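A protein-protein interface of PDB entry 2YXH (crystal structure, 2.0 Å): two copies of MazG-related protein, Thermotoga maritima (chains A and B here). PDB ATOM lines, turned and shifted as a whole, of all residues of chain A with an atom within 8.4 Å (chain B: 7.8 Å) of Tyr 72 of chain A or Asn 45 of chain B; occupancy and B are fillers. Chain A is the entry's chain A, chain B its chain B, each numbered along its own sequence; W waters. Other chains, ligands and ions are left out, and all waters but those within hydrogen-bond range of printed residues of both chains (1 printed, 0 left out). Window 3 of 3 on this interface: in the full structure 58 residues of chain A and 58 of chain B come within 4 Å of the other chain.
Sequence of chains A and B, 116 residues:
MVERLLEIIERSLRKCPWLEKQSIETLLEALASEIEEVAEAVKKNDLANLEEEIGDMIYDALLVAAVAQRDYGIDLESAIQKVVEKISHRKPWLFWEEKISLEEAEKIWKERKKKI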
ATOM      1  N   SER A  23     -36.239  10.290  -0.121  1.00  0.00           N
ATOM      2  CA  SER A  23     -35.002  10.784   0.490  1.00  0.00           C
ATOM      3  C   SER A  23     -35.078  10.501   1.993  1.00  0.00           C
ATOM      4  O   SER A  23     -36.154  10.286   2.565  1.00  0.00           O
ATOM      5  CB  SER A  23     -34.864  12.292   0.280  1.00  0.00           C
ATOM      6  OG  SER A  23     -35.893  12.911   1.000  1.00  0.00           O
ATOM      7  N   ILE A  24     -33.927  10.497   2.633  1.00  0.00           N
ATOM      8  CA  ILE A  24     -33.846  10.324   4.091  1.00  0.00           C
ATOM      9  C   ILE A  24     -34.708  11.306   4.838  1.00  0.00           C
ATOM     10  O   ILE A  24     -35.407  10.960   5.777  1.00  0.00           O
ATOM     11  CB  ILE A  24     -32.349  10.262   4.575  1.00  0.00           C
ATOM     12  CG1 ILE A  24     -32.224   9.540   5.913  1.00  0.00           C
ATOM     13  CG2 ILE A  24     -31.665  11.593   4.550  1.00  0.00           C
ATOM     14  CD1 ILE A  24     -30.787   9.131   6.200  1.00  0.00           C
ATOM     15  N   GLU A  25     -34.700  12.535   4.372  1.00  0.00           N
ATOM     16  CA  GLU A  25     -35.636  13.563   4.818  1.00  0.00           C
ATOM     17  C   GLU A  25     -37.072  13.121   4.812  1.00  0.00           C
ATOM     18  O   GLU A  25     -37.791  13.246   5.787  1.00  0.00           O
ATOM     19  CB  GLU A  25     -35.493  14.797   3.933  1.00  0.00           C
ATOM     20  CG  GLU A  25     -34.206  15.623   4.272  1.00  0.00           C
ATOM     21  CD  GLU A  25     -33.044  15.472   3.263  1.00  0.00           C
ATOM     22  OE1 GLU A  25     -32.982  14.495   2.484  1.00  0.00           O
ATOM     23  OE2 GLU A  25     -32.179  16.394   3.250  1.00  0.00           O
ATOM     24  N   VAL A  64     -35.156   4.446   7.570  1.00  0.00           N
ATOM     25  CA  VAL A  64     -34.224   5.604   7.593  1.00  0.00           C
ATOM     26  C   VAL A  64     -32.785   5.005   7.611  1.00  0.00           C
ATOM     27  O   VAL A  64     -31.921   5.363   6.790  1.00  0.00           O
ATOM     28  CB  VAL A  64     -34.520   6.591   8.740  1.00  0.00           C
ATOM     29  CG1 VAL A  64     -33.443   7.647   8.885  1.00  0.00           C
ATOM     30  CG2 VAL A  64     -35.893   7.258   8.593  1.00  0.00           C
ATOM     31  N   ALA A  65     -32.515   4.057   8.489  1.00  0.00           N
ATOM     32  CA  ALA A  65     -31.223   3.412   8.424  1.00  0.00           C
ATOM     33  C   ALA A  65     -30.872   3.020   6.990  1.00  0.00           C
ATOM     34  O   ALA A  65     -29.786   3.380   6.486  1.00  0.00           O
ATOM     35  CB  ALA A  65     -31.119   2.199   9.374  1.00  0.00           C
ATOM     36  N   ALA A  66     -31.732   2.280   6.328  1.00  0.00           N
ATOM     37  CA  ALA A  66     -31.469   1.846   4.913  1.00  0.00           C
ATOM     38  C   ALA A  66     -31.020   2.901   3.903  1.00  0.00           C
ATOM     39  O   ALA A  66     -30.118   2.658   3.056  1.00  0.00           O
ATOM     40  CB  ALA A  66     -32.663   1.038   4.333  1.00  0.00           C
ATOM     41  N   VAL A  67     -31.631   4.096   3.983  1.00  0.00           N
ATOM     42  CA  VAL A  67     -31.361   5.069   3.003  1.00  0.00           C
ATOM     43  C   VAL A  67     -30.125   5.875   3.425  1.00  0.00           C
ATOM     44  O   VAL A  67     -29.452   6.461   2.572  1.00  0.00           O
ATOM     45  CB  VAL A  67     -32.582   6.044   2.833  1.00  0.00           C
ATOM     46  CG1 VAL A  67     -32.187   7.230   1.945  1.00  0.00           C
ATOM     47  CG2 VAL A  67     -33.861   5.258   2.207  1.00  0.00           C
ATOM     48  N   ALA A  68     -29.860   5.921   4.740  1.00  0.00           N
ATOM     49  CA  ALA A  68     -28.577   6.410   5.278  1.00  0.00           C
ATOM     50  C   ALA A  68     -27.443   5.538   4.671  1.00  0.00           C
ATOM     51  O   ALA A  68     -26.401   6.066   4.304  1.00  0.00           O
ATOM     52  CB  ALA A  68     -28.549   6.352   6.751  1.00  0.00           C
ATOM     53  N   GLN A  69     -27.633   4.227   4.561  1.00  0.00           N
ATOM     54  CA  GLN A  69     -26.668   3.384   3.861  1.00  0.00           C
ATOM     55  C   GLN A  69     -26.669   3.678   2.350  1.00  0.00           C
ATOM     56  O   GLN A  69     -25.618   3.771   1.743  1.00  0.00           O
ATOM     57  CB  GLN A  69     -26.973   1.904   4.055  1.00  0.00           C
ATOM     58  CG  GLN A  69     -26.064   0.985   3.285  1.00  0.00           C
ATOM     59  CD  GLN A  69     -26.543  -0.556   3.276  1.00  0.00           C
ATOM     60  OE1 GLN A  69     -27.548  -0.963   2.630  1.00  0.00           O
ATOM     61  NE2 GLN A  69     -25.799  -1.361   3.969  1.00  0.00           N
ATOM     62  N   ARG A  70     -27.850   3.776   1.752  1.00  0.00           N
ATOM     63  CA  ARG A  70     -27.979   3.945   0.324  1.00  0.00           C
ATOM     64  C   ARG A  70     -27.263   5.212  -0.173  1.00  0.00           C
ATOM     65  O   ARG A  70     -26.438   5.205  -1.124  1.00  0.00           O
ATOM     66  CB  ARG A  70     -29.470   4.111  -0.037  1.00  0.00           C
ATOM     67  CG  ARG A  70     -29.694   3.873  -1.505  1.00  0.00           C
ATOM     68  CD  ARG A  70     -31.083   4.279  -1.909  1.00  0.00           C
ATOM     69  NE  ARG A  70     -31.425   5.709  -1.662  1.00  0.00           N
ATOM     70  CZ  ARG A  70     -32.662   6.128  -1.572  1.00  0.00           C
ATOM     71  NH1 ARG A  70     -33.675   5.230  -1.686  1.00  0.00           N
ATOM     72  NH2 ARG A  70     -32.881   7.416  -1.354  1.00  0.00           N
ATOM     73  N   ASP A  71     -27.664   6.298   0.450  1.00  0.00           N
ATOM     74  CA  ASP A  71     -27.241   7.614   0.066  1.00  0.00           C
ATOM     75  C   ASP A  71     -25.931   8.120   0.722  1.00  0.00           C
ATOM     76  O   ASP A  71     -25.323   8.998   0.181  1.00  0.00           O
ATOM     77  CB  ASP A  71     -28.360   8.613   0.304  1.00  0.00           C
ATOM     78  CG  ASP A  71     -29.518   8.411  -0.683  1.00  0.00           C
ATOM     79  OD1 ASP A  71     -29.454   7.506  -1.534  1.00  0.00           O
ATOM     80  OD2 ASP A  71     -30.524   9.142  -0.576  1.00  0.00           O
ATOM     81  N   TYR A  72     -25.613   7.688   1.933  1.00  0.00           N
ATOM     82  CA  TYR A  72     -24.546   8.325   2.711  1.00  0.00           C
ATOM     83  C   TYR A  72     -23.480   7.266   3.062  1.00  0.00           C
ATOM     84  O   TYR A  72     -22.495   7.568   3.717  1.00  0.00           O
ATOM     85  CB  TYR A  72     -25.042   9.084   3.913  1.00  0.00           C
ATOM     86  CG  TYR A  72     -25.901  10.283   3.486  1.00  0.00           C
ATOM     87  CD1 TYR A  72     -25.290  11.503   3.165  1.00  0.00           C
ATOM     88  CD2 TYR A  72     -27.300  10.209   3.424  1.00  0.00           C
ATOM     89  CE1 TYR A  72     -26.063  12.613   2.680  1.00  0.00           C
ATOM     90  CE2 TYR A  72     -28.115  11.349   2.928  1.00  0.00           C
ATOM     91  CZ  TYR A  72     -27.439  12.525   2.563  1.00  0.00           C
ATOM     92  OH  TYR A  72     -28.143  13.680   2.090  1.00  0.00           O
ATOM     93  N   GLY A  73     -23.724   6.040   2.622  1.00  0.00           N
ATOM     94  CA  GLY A  73     -22.875   4.848   2.845  1.00  0.00           C
ATOM     95  C   GLY A  73     -22.788   4.418   4.305  1.00  0.00           C
ATOM     96  O   GLY A  73     -21.970   3.565   4.671  1.00  0.00           O
ATOM     97  N   ILE A  74     -23.700   4.883   5.146  1.00  0.00           N
ATOM     98  CA  ILE A  74     -23.706   4.439   6.566  1.00  0.00           C
ATOM     99  C   ILE A  74     -23.952   2.910   6.748  1.00  0.00           C
ATOM    100  O   ILE A  74     -24.992   2.371   6.381  1.00  0.00           O
ATOM    101  CB  ILE A  74     -24.775   5.186   7.430  1.00  0.00           C
ATOM    102  CG1 ILE A  74     -24.700   6.722   7.295  1.00  0.00           C
ATOM    103  CG2 ILE A  74     -24.587   4.857   8.871  1.00  0.00           C
ATOM    104  CD1 ILE A  74     -23.289   7.373   7.629  1.00  0.00           C
ATOM    105  N   ASP A  75     -23.046   2.230   7.406  1.00  0.00           N
ATOM    106  CA  ASP A  75     -23.212   0.797   7.640  1.00  0.00           C
ATOM    107  C   ASP A  75     -24.007   0.662   8.952  1.00  0.00           C
ATOM    108  O   ASP A  75     -23.619   1.256   9.920  1.00  0.00           O
ATOM    109  CB  ASP A  75     -21.816   0.256   7.835  1.00  0.00           C
ATOM    110  CG  ASP A  75     -21.766  -1.230   8.015  1.00  0.00           C
ATOM    111  OD1 ASP A  75     -22.757  -1.947   7.893  1.00  0.00           O
ATOM    112  OD2 ASP A  75     -20.659  -1.696   8.237  1.00  0.00           O
ATOM    113  N   ALA B  39     -31.670  14.573  11.159  1.00  0.00           N
ATOM    114  CA  ALA B  39     -31.965  15.469  10.061  1.00  0.00           C
ATOM    115  C   ALA B  39     -30.795  16.461   9.951  1.00  0.00           C
ATOM    116  O   ALA B  39     -30.282  16.761   8.865  1.00  0.00           O
ATOM    117  CB  ALA B  39     -33.298  16.151  10.265  1.00  0.00           C
ATOM    118  N   GLU B  40     -30.325  16.900  11.101  1.00  0.00           N
ATOM    119  CA  GLU B  40     -29.172  17.799  11.168  1.00  0.00           C
ATOM    120  C   GLU B  40     -27.846  17.251  10.624  1.00  0.00           C
ATOM    121  O   GLU B  40     -27.169  17.928   9.854  1.00  0.00           O
ATOM    122  CB  GLU B  40     -29.056  18.327  12.597  1.00  0.00           C
ATOM    123  CG  GLU B  40     -27.860  19.144  12.914  1.00  0.00           C
ATOM    124  CD  GLU B  40     -28.024  20.581  12.456  1.00  0.00           C
ATOM    125  OE1 GLU B  40     -29.148  20.949  12.026  1.00  0.00           O
ATOM    126  OE2 GLU B  40     -27.011  21.319  12.513  1.00  0.00           O
ATOM    127  N   ALA B  41     -27.431  16.036  10.990  1.00  0.00           N
ATOM    128  CA  ALA B  41     -26.194  15.520  10.435  1.00  0.00           C
ATOM    129  C   ALA B  41     -26.316  15.314   8.909  1.00  0.00           C
ATOM    130  O   ALA B  41     -25.306  15.387   8.189  1.00  0.00           O
ATOM    131  CB  ALA B  41     -25.719  14.258  11.137  1.00  0.00           C
ATOM    132  N   VAL B  42     -27.531  15.062   8.423  1.00  0.00           N
ATOM    133  CA  VAL B  42     -27.765  14.993   6.970  1.00  0.00           C
ATOM    134  C   VAL B  42     -27.518  16.371   6.304  1.00  0.00           C
ATOM    135  O   VAL B  42     -26.772  16.432   5.337  1.00  0.00           O
ATOM    136  CB  VAL B  42     -29.178  14.422   6.616  1.00  0.00           C
ATOM    137  CG1 VAL B  42     -29.520  14.555   5.128  1.00  0.00           C
ATOM    138  CG2 VAL B  42     -29.257  13.011   7.049  1.00  0.00           C
ATOM    139  N   LYS B  43     -28.160  17.427   6.817  1.00  0.00           N
ATOM    140  CA  LYS B  43     -27.913  18.786   6.399  1.00  0.00           C
ATOM    141  C   LYS B  43     -26.446  19.107   6.121  1.00  0.00           C
ATOM    142  O   LYS B  43     -26.118  19.780   5.158  1.00  0.00           O
ATOM    143  CB  LYS B  43     -28.352  19.734   7.489  1.00  0.00           C
ATOM    144  CG  LYS B  43     -29.626  20.445   7.208  1.00  0.00           C
ATOM    145  CD  LYS B  43     -30.183  21.116   8.497  1.00  0.00           C
ATOM    146  CE  LYS B  43     -31.363  20.324   9.200  1.00  0.00           C
ATOM    147  NZ  LYS B  43     -32.777  20.552   8.655  1.00  0.00           N
ATOM    148  N   LYS B  44     -25.576  18.606   6.975  1.00  0.00           N
ATOM    149  CA  LYS B  44     -24.220  19.033   7.028  1.00  0.00           C
ATOM    150  C   LYS B  44     -23.331  17.962   6.486  1.00  0.00           C
ATOM    151  O   LYS B  44     -22.148  17.989   6.675  1.00  0.00           O
ATOM    152  CB  LYS B  44     -23.893  19.382   8.495  1.00  0.00           C
ATOM    153  CG  LYS B  44     -24.463  20.780   8.815  1.00  0.00           C
ATOM    154  CD  LYS B  44     -24.804  21.054  10.263  1.00  0.00           C
ATOM    155  CE  LYS B  44     -24.950  22.619  10.522  1.00  0.00           C
ATOM    156  NZ  LYS B  44     -26.251  23.156   9.944  1.00  0.00           N
ATOM    157  N   ASN B  45     -23.906  17.009   5.777  1.00  0.00           N
ATOM    158  CA  ASN B  45     -23.145  15.856   5.257  1.00  0.00           C
ATOM    159  C   ASN B  45     -22.049  15.492   6.211  1.00  0.00           C
ATOM    160  O   ASN B  45     -20.905  15.327   5.803  1.00  0.00           O
ATOM    161  CB  ASN B  45     -22.581  16.078   3.826  1.00  0.00           C
ATOM    162  CG  ASN B  45     -23.639  16.588   2.851  1.00  0.00           C
ATOM    163  OD1 ASN B  45     -23.484  17.642   2.242  1.00  0.00           O
ATOM    164  ND2 ASN B  45     -24.732  15.864   2.739  1.00  0.00           N
ATOM    165  N   ASP B  46     -22.407  15.399   7.495  1.00  0.00           N
ATOM    166  CA  ASP B  46     -21.485  15.010   8.549  1.00  0.00           C
ATOM    167  C   ASP B  46     -21.661  13.536   8.748  1.00  0.00           C
ATOM    168  O   ASP B  46     -22.594  13.092   9.434  1.00  0.00           O
ATOM    169  CB  ASP B  46     -21.792  15.791   9.834  1.00  0.00           C
ATOM    170  CG  ASP B  46     -20.734  15.553  10.946  1.00  0.00           C
ATOM    171  OD1 ASP B  46     -19.995  14.513  10.965  1.00  0.00           O
ATOM    172  OD2 ASP B  46     -20.670  16.437  11.848  1.00  0.00           O
ATOM    173  N   LEU B  47     -20.778  12.780   8.119  1.00  0.00           N
ATOM    174  CA  LEU B  47     -20.870  11.293   8.046  1.00  0.00           C
ATOM    175  C   LEU B  47     -20.693  10.512   9.337  1.00  0.00           C
ATOM    176  O   LEU B  47     -21.435   9.543   9.621  1.00  0.00           O
ATOM    177  CB  LEU B  47     -19.906  10.735   6.988  1.00  0.00           C
ATOM    178  CG  LEU B  47     -20.038  11.121   5.510  1.00  0.00           C
ATOM    179  CD1 LEU B  47     -18.992  10.297   4.658  1.00  0.00           C
ATOM    180  CD2 LEU B  47     -21.522  10.905   5.022  1.00  0.00           C
ATOM    181  N   ALA B  48     -19.620  10.839  10.036  1.00  0.00           N
ATOM    182  CA  ALA B  48     -19.386  10.416  11.411  1.00  0.00           C
ATOM    183  C   ALA B  48     -20.552  10.750  12.371  1.00  0.00           C
ATOM    184  O   ALA B  48     -20.914   9.962  13.219  1.00  0.00           O
ATOM    185  CB  ALA B  48     -18.132  11.125  11.899  1.00  0.00           C
ATOM    186  N   ASN B  49     -21.100  11.952  12.278  1.00  0.00           N
ATOM    187  CA  ASN B  49     -22.218  12.244  13.127  1.00  0.00           C
ATOM    188  C   ASN B  49     -23.479  11.456  12.659  1.00  0.00           C
ATOM    189  O   ASN B  49     -24.262  10.950  13.494  1.00  0.00           O
ATOM    190  CB  ASN B  49     -22.504  13.705  13.163  1.00  0.00           C
ATOM    191  CG  ASN B  49     -23.556  14.057  14.207  1.00  0.00           C
ATOM    192  OD1 ASN B  49     -23.400  13.744  15.404  1.00  0.00           O
ATOM    193  ND2 ASN B  49     -24.636  14.710  13.777  1.00  0.00           N
ATOM    194  N   LEU B  50     -23.647  11.277  11.344  1.00  0.00           N
ATOM    195  CA  LEU B  50     -24.829  10.566  10.869  1.00  0.00           C
ATOM    196  C   LEU B  50     -24.812   9.110  11.409  1.00  0.00           C
ATOM    197  O   LEU B  50     -25.817   8.557  11.896  1.00  0.00           O
ATOM    198  CB  LEU B  50     -24.964  10.662   9.319  1.00  0.00           C
ATOM    199  CG  LEU B  50     -26.169   9.969   8.575  1.00  0.00           C
ATOM    200  CD1 LEU B  50     -27.492  10.431   9.132  1.00  0.00           C
ATOM    201  CD2 LEU B  50     -26.144  10.300   7.114  1.00  0.00           C
ATOM    202  N   GLU B  51     -23.646   8.530  11.341  1.00  0.00           N
ATOM    203  CA  GLU B  51     -23.514   7.198  11.805  1.00  0.00           C
ATOM    204  C   GLU B  51     -23.890   7.188  13.265  1.00  0.00           C
ATOM    205  O   GLU B  51     -24.466   6.183  13.750  1.00  0.00           O
ATOM    206  CB  GLU B  51     -22.099   6.747  11.709  1.00  0.00           C
ATOM    207  CG  GLU B  51     -21.982   5.212  11.951  1.00  0.00           C
ATOM    208  CD  GLU B  51     -20.578   4.789  11.900  1.00  0.00           C
ATOM    209  OE1 GLU B  51     -19.803   5.595  12.505  1.00  0.00           O
ATOM    210  OE2 GLU B  51     -20.260   3.703  11.285  1.00  0.00           O
ATOM    211  N   ILE B  54     -27.795   7.819  13.589  1.00  0.00           N
ATOM    212  CA  ILE B  54     -28.560   6.659  13.126  1.00  0.00           C
ATOM    213  C   ILE B  54     -28.650   5.644  14.270  1.00  0.00           C
ATOM    214  O   ILE B  54     -29.717   5.221  14.630  1.00  0.00           O
ATOM    215  CB  ILE B  54     -28.019   6.067  11.835  1.00  0.00           C
ATOM    216  CG1 ILE B  54     -28.319   7.096  10.676  1.00  0.00           C
ATOM    217  CG2 ILE B  54     -28.692   4.724  11.533  1.00  0.00           C
ATOM    218  CD1 ILE B  54     -29.754   7.141  10.300  1.00  0.00           C
HETATM  219  O   HOH W   1     -28.102  17.019   2.503  1.00  0.00           O
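O of Ala 68 of chain A lies within hydrogen-bond range of N of Ile 74 of chain A. O of Val 42 of chain B lies within hydrogen-bond range of ND2 of Asn 45 of chain B (3.4 Å). O of Ala 68 of chain A sits at hydrogen-bond distance from N of Gly 73 of chain A.
Ile 24 of chain A touches Val 42 of chain B. Glu 25 of chain A touches Val 42 of chain B. CG1 of Val 64 of chain A touches CD1 of Ile 54 of chain B (3.98 Å). Ala 68 of chain A touches Ile 54 of chain B. CG1 of Val 42 of chain B touches OH of Tyr 72 of chain A, at 3.4 Å. ND2 of Asn 45 of chain B touches CE1 of Tyr 72 of chain A (3.5 Å). Leu 47 of chain B touches Tyr 72 of chain A. O of Leu 47 of chain B touches CD1 of Ile 74 of chain A, 3.5 Å away. Leu 50 of chain B touches Ile 74 of chain A. Ile 74 of chain A touches Glu 51 of chain B (CG2 to CA, 3.9 Å).
Hydrophobic or aromatic side chains of chain B that line the printed part of chain A: Val 42, Leu 47, Leu 50 and Ile 54. Hydrophobic or aromatic side chains of chain A that line the printed part of chain B: Ile 24, Val 64, Ala 68, Tyr 72 and Ile 74. Among the printed residues, 11 pairs touch across the chains. Among the printed residues, no Asp or Glu carboxylate lies within 4 Å of a Lys or Arg side-chain nitrogen of the other chain.
Printed residues of chain B within 4 Å of Ile 24 of chain A: Val 42 (3.7 Å). Printed residues of chain B within 4 Å of Ala 68 of chain A: Ile 54 (3.8 Å). Tyr 72 of chain A touches four residues of chain B. Of the printed residues of chain A, Val 42 of chain B touches Ile 24, Glu 25 and Tyr 72. Asn 45 of chain B touches one residue of chain A. Printed residues of chain A within 4 Å of Leu 47 of chain B: Tyr 72 (3.7 Å) and Ile 74 (3.5 Å). The nearest residue of chain A that does not touch Asn 45 of chain B is Asp 71 of chain A (7.4 Å).
No position is printed for both chains.
Water W1 lies within hydrogen-bond range of O of Val 42 of chain B (3.2 Å) and OH of Tyr 72 of chain A (3.4 Å).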
